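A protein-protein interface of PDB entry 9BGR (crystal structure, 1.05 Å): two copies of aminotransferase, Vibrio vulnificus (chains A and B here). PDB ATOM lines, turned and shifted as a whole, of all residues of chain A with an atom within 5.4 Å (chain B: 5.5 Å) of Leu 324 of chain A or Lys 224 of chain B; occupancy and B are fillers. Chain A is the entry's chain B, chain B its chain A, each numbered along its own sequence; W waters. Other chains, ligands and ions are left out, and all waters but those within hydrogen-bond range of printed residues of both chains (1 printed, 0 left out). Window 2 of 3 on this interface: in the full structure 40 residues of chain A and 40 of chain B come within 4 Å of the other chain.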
ATOM      1  N   THR A  81      19.041  11.333  16.558  1.00  0.00           N
ATOM      2  CA  THR A  81      18.112  11.541  15.452  1.00  0.00           C
ATOM      3  C   THR A  81      18.814  11.947  14.157  1.00  0.00           C
ATOM      4  O   THR A  81      18.287  11.689  13.076  1.00  0.00           O
ATOM      5  CB  THR A  81      17.041  12.543  15.880  1.00  0.00           C
ATOM      6  OG1 THR A  81      16.572  12.088  17.156  1.00  0.00           O
ATOM      7  CG2 THR A  81      15.901  12.619  14.889  1.00  0.00           C
ATOM      8  N   ASN A  85      17.622  11.519  10.266  1.00  0.00           N
ATOM      9  CA  ASN A  85      17.258  12.787   9.661  1.00  0.00           C
ATOM     10  C   ASN A  85      18.056  13.043   8.392  1.00  0.00           C
ATOM     11  O   ASN A  85      17.521  13.512   7.402  1.00  0.00           O
ATOM     12  CB  ASN A  85      17.578  13.968  10.584  1.00  0.00           C
ATOM     13  CG  ASN A  85      16.517  14.257  11.614  1.00  0.00           C
ATOM     14  OD1 ASN A  85      15.448  13.668  11.603  1.00  0.00           O
ATOM     15  ND2 ASN A  85      16.791  15.229  12.471  1.00  0.00           N
ATOM     16  N   GLU A  88      16.865  11.347   5.323  1.00  0.00           N
ATOM     17  CA  GLU A  88      15.675  11.979   4.794  1.00  0.00           C
ATOM     18  C   GLU A  88      15.992  13.318   4.126  1.00  0.00           C
ATOM     19  O   GLU A  88      15.367  13.697   3.138  1.00  0.00           O
ATOM     20  CB  GLU A  88      14.615  12.132   5.879  1.00  0.00           C
ATOM     21  CG  GLU A  88      14.111  10.824   6.444  1.00  0.00           C
ATOM     22  CD  GLU A  88      13.056  10.081   5.634  1.00  0.00           C
ATOM     23  OE1 GLU A  88      12.318  10.748   4.890  1.00  0.00           O
ATOM     24  OE2 GLU A  88      12.977   8.852   5.777  1.00  0.00           O
ATOM     25  N   MET A 319      14.312   5.820  16.733  1.00  0.00           N
ATOM     26  CA  MET A 319      13.838   6.446  15.503  1.00  0.00           C
ATOM     27  C   MET A 319      12.366   6.106  15.245  1.00  0.00           C
ATOM     28  O   MET A 319      11.612   6.971  14.811  1.00  0.00           O
ATOM     29  CB  MET A 319      14.713   6.036  14.309  1.00  0.00           C
ATOM     30  CG  MET A 319      16.207   6.418  14.414  1.00  0.00           C
ATOM     31  SD  MET A 319      16.495   8.175  14.681  1.00  0.00           S
ATOM     32  CE  MET A 319      16.585   8.263  16.460  1.00  0.00           C
ATOM     33  N   LEU A 322       9.660   8.353  16.953  1.00  0.00           N
ATOM     34  CA  LEU A 322       9.620   9.795  16.759  1.00  0.00           C
ATOM     35  C   LEU A 322       8.537  10.245  15.785  1.00  0.00           C
ATOM     36  O   LEU A 322       8.232  11.426  15.719  1.00  0.00           O
ATOM     37  CB  LEU A 322      10.986  10.284  16.269  1.00  0.00           C
ATOM     38  CG  LEU A 322      12.134  10.057  17.250  1.00  0.00           C
ATOM     39  CD1 LEU A 322      13.399  10.663  16.703  1.00  0.00           C
ATOM     40  CD2 LEU A 322      11.810  10.580  18.643  1.00  0.00           C
ATOM     41  N   GLY A 323       7.992   9.329  14.978  1.00  0.00           N
ATOM     42  CA  GLY A 323       6.986   9.706  13.993  1.00  0.00           C
ATOM     43  C   GLY A 323       7.493  10.496  12.785  1.00  0.00           C
ATOM     44  O   GLY A 323       6.687  11.102  12.069  1.00  0.00           O
ATOM     45  N   LEU A 324       8.798  10.408  12.501  1.00  0.00           N
ATOM     46  CA  LEU A 324       9.427  11.160  11.431  1.00  0.00           C
ATOM     47  C   LEU A 324       9.801  10.301  10.228  1.00  0.00           C
ATOM     48  O   LEU A 324      10.019  10.844   9.154  1.00  0.00           O
ATOM     49  CB  LEU A 324      10.687  11.843  11.945  1.00  0.00           C
ATOM     50  CG  LEU A 324      10.476  12.896  13.019  1.00  0.00           C
ATOM     51  CD1 LEU A 324      11.827  13.422  13.486  1.00  0.00           C
ATOM     52  CD2 LEU A 324       9.590  14.027  12.507  1.00  0.00           C
ATOM     53  N   PHE A 325       9.946   8.997  10.441  1.00  0.00           N
ATOM     54  CA  PHE A 325      10.522   8.089   9.463  1.00  0.00           C
ATOM     55  C   PHE A 325       9.451   7.075   9.094  1.00  0.00           C
ATOM     56  O   PHE A 325       9.416   5.977   9.647  1.00  0.00           O
ATOM     57  CB  PHE A 325      11.783   7.452  10.026  1.00  0.00           C
ATOM     58  CG  PHE A 325      12.703   8.503  10.586  1.00  0.00           C
ATOM     59  CD1 PHE A 325      13.284   9.447   9.753  1.00  0.00           C
ATOM     60  CD2 PHE A 325      12.933   8.608  11.946  1.00  0.00           C
ATOM     61  CE1 PHE A 325      14.053  10.480  10.267  1.00  0.00           C
ATOM     62  CE2 PHE A 325      13.682   9.650  12.469  1.00  0.00           C
ATOM     63  CZ  PHE A 325      14.224  10.593  11.620  1.00  0.00           C
ATOM     64  N   ASN A 326       8.576   7.454   8.155  1.00  0.00           N
ATOM     65  CA  ASN A 326       7.299   6.766   8.030  1.00  0.00           C
ATOM     66  C   ASN A 326       7.258   5.843   6.820  1.00  0.00           C
ATOM     67  O   ASN A 326       6.179   5.430   6.381  1.00  0.00           O
ATOM     68  CB  ASN A 326       6.157   7.771   8.087  1.00  0.00           C
ATOM     69  CG  ASN A 326       6.161   8.513   9.403  1.00  0.00           C
ATOM     70  OD1 ASN A 326       6.293   7.925  10.479  1.00  0.00           O
ATOM     71  ND2 ASN A 326       6.159   9.827   9.325  1.00  0.00           N
ATOM     72  N   LEU B 208      14.304  25.114  14.155  1.00  0.00           N
ATOM     73  CA  LEU B 208      14.220  23.664  14.170  1.00  0.00           C
ATOM     74  C   LEU B 208      15.240  23.073  13.184  1.00  0.00           C
ATOM     75  O   LEU B 208      15.974  22.136  13.501  1.00  0.00           O
ATOM     76  CB  LEU B 208      12.808  23.223  13.756  1.00  0.00           C
ATOM     77  CG  LEU B 208      11.661  23.518  14.723  1.00  0.00           C
ATOM     78  CD1 LEU B 208      10.346  23.108  14.089  1.00  0.00           C
ATOM     79  CD2 LEU B 208      11.856  22.826  16.055  1.00  0.00           C
ATOM     80  N   GLY B 213      15.778  19.421  14.137  1.00  0.00           N
ATOM     81  CA  GLY B 213      14.354  19.454  14.420  1.00  0.00           C
ATOM     82  C   GLY B 213      14.016  19.553  15.905  1.00  0.00           C
ATOM     83  O   GLY B 213      12.859  19.355  16.286  1.00  0.00           O
ATOM     84  N   MET B 214      14.990  19.912  16.753  1.00  0.00           N
ATOM     85  CA  MET B 214      14.794  19.891  18.207  1.00  0.00           C
ATOM     86  C   MET B 214      14.036  21.127  18.689  1.00  0.00           C
ATOM     87  O   MET B 214      14.408  22.261  18.395  1.00  0.00           O
ATOM     88  CB  MET B 214      16.136  19.835  18.941  1.00  0.00           C
ATOM     89  CG  MET B 214      16.859  18.519  18.719  1.00  0.00           C
ATOM     90  SD  MET B 214      18.636  18.530  19.155  1.00  0.00           S
ATOM     91  CE  MET B 214      18.552  18.694  20.935  1.00  0.00           C
ATOM     92  N   GLN B 215      12.989  20.873  19.473  1.00  0.00           N
ATOM     93  CA  GLN B 215      12.249  21.896  20.194  1.00  0.00           C
ATOM     94  C   GLN B 215      12.377  21.595  21.687  1.00  0.00           C
ATOM     95  O   GLN B 215      12.044  20.501  22.132  1.00  0.00           O
ATOM     96  CB  GLN B 215      10.795  21.861  19.705  1.00  0.00           C
ATOM     97  CG  GLN B 215       9.865  22.859  20.379  1.00  0.00           C
ATOM     98  CD  GLN B 215       8.439  22.629  19.942  1.00  0.00           C
ATOM     99  OE1 GLN B 215       7.767  21.708  20.405  1.00  0.00           O
ATOM    100  NE2 GLN B 215       7.977  23.444  19.008  1.00  0.00           N
ATOM    101  N   VAL B 222      11.717  17.638  22.104  1.00  0.00           N
ATOM    102  CA  VAL B 222      10.897  16.970  21.107  1.00  0.00           C
ATOM    103  C   VAL B 222      11.551  17.195  19.748  1.00  0.00           C
ATOM    104  O   VAL B 222      11.941  18.310  19.416  1.00  0.00           O
ATOM    105  CB  VAL B 222       9.454  17.519  21.123  1.00  0.00           C
ATOM    106  CG1 VAL B 222       8.580  16.865  20.065  1.00  0.00           C
ATOM    107  CG2 VAL B 222       8.815  17.403  22.503  1.00  0.00           C
ATOM    108  N   PHE B 223      11.583  16.129  18.948  1.00  0.00           N
ATOM    109  CA  PHE B 223      12.037  16.196  17.567  1.00  0.00           C
ATOM    110  C   PHE B 223      10.822  16.415  16.678  1.00  0.00           C
ATOM    111  O   PHE B 223      10.038  15.498  16.456  1.00  0.00           O
ATOM    112  CB  PHE B 223      12.842  14.945  17.202  1.00  0.00           C
ATOM    113  CG  PHE B 223      14.142  14.853  17.961  1.00  0.00           C
ATOM    114  CD1 PHE B 223      14.192  14.240  19.199  1.00  0.00           C
ATOM    115  CD2 PHE B 223      15.311  15.358  17.434  1.00  0.00           C
ATOM    116  CE1 PHE B 223      15.379  14.200  19.916  1.00  0.00           C
ATOM    117  CE2 PHE B 223      16.499  15.284  18.141  1.00  0.00           C
ATOM    118  CZ  PHE B 223      16.531  14.696  19.372  1.00  0.00           C
ATOM    119  N   LYS B 224      10.674  17.640  16.175  1.00  0.00           N
ATOM    120  CA  LYS B 224       9.453  18.021  15.487  1.00  0.00           C
ATOM    121  C   LYS B 224       9.482  17.683  13.998  1.00  0.00           C
ATOM    122  O   LYS B 224       8.428  17.524  13.376  1.00  0.00           O
ATOM    123  CB  LYS B 224       9.220  19.521  15.617  1.00  0.00           C
ATOM    124  CG  LYS B 224       8.831  19.975  17.005  1.00  0.00           C
ATOM    125  CD  LYS B 224       7.541  19.406  17.516  1.00  0.00           C
ATOM    126  CE  LYS B 224       6.366  19.726  16.619  1.00  0.00           C
ATOM    127  NZ  LYS B 224       5.091  19.699  17.376  1.00  0.00           N
ATOM    128  N   CYS B 225      10.672  17.726  13.395  1.00  0.00           N
ATOM    129  CA  CYS B 225      10.815  17.540  11.967  1.00  0.00           C
ATOM    130  C   CYS B 225      12.240  17.083  11.683  1.00  0.00           C
ATOM    131  O   CYS B 225      13.118  17.191  12.531  1.00  0.00           O
ATOM    132  CB  CYS B 225      10.493  18.818  11.204  1.00  0.00           C
ATOM    133  SG  CYS B 225      11.601  20.202  11.567  1.00  0.00           S
ATOM    134  N   VAL B 226      12.501  16.626  10.466  1.00  0.00           N
ATOM    135  CA  VAL B 226      13.872  16.331  10.078  1.00  0.00           C
ATOM    136  C   VAL B 226      14.621  17.643   9.867  1.00  0.00           C
ATOM    137  O   VAL B 226      14.072  18.631   9.379  1.00  0.00           O
ATOM    138  CB  VAL B 226      13.933  15.399   8.852  1.00  0.00           C
ATOM    139  CG1 VAL B 226      13.261  14.074   9.139  1.00  0.00           C
ATOM    140  CG2 VAL B 226      13.397  16.000   7.580  1.00  0.00           C
HETATM  141  O   HOH W   1       9.096  13.243  17.598  1.00  0.00           O
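The backbone carbonyl oxygen (O) of Gly 213 of chain B sits at hydrogen-bond distance from the backbone NH (N) of Lys 224 of chain B, at 2.8 Å.
CE2 of Phe 223 of chain B touches OG1 of Thr 81 of chain A, 3.3 Å away. OD1 of Asn 85 of chain A touches CG1 of Val 226 of chain B, 3.3 Å away. Leu 324 of chain A touches Lys 224 of chain B. Leu 324 of chain A touches Cys 225 of chain B (CD2 to CA, 3.8 Å). Val 226 of chain B touches Phe 325 of chain A (CG1 to CE1, 3.8 Å).
Printed residues of chain B within 4 Å of Thr 81 of chain A: Phe 223 (3.3 Å). Leu 324 of chain A touches just these residues of chain B: Lys 224 (3.8 Å) and Cys 225 (3.8 Å). Lys 224 of chain B touches just one residue of chain A: Leu 324. Printed residues of chain A within 4 Å of Cys 225 of chain B: Leu 324 (3.8 Å). The nearest residue of chain B that does not touch Leu 324 of chain A is Phe 223 of chain B (4.04 Å). The nearest printed residue of chain A that does not touch Lys 224 of chain B is Leu 322 of chain A (6.5 Å).
Printed residues of chain B that touch a printed residue of chain A: Phe 223, Lys 224, Cys 225 and Val 226. Along chain B the printed residues that touch a printed residue of chain A span positions 223 to 226. Printed residues of chain A that touch a printed residue of chain B: Thr 81, Asn 85, Leu 324 and Phe 325. Hydrophobic or aromatic side chains of chain A within 4 Å of the printed part of chain B: Leu 324 and Phe 325. Among the printed residues, 5 pairs touch across the chains. Among the printed residues, no Asp or Glu carboxylate lies within 4 Å of a Lys or Arg side-chain nitrogen of the other chain.
No position is printed for both chains. Of the 5 pairs that touch across the chains among the printed residues, none has its exchanged pair printed and touching as well.
Water W1 bridges the backbone carbonyl oxygen of Phe 223 of chain B and the backbone carbonyl oxygen of Leu 322 of chain A.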
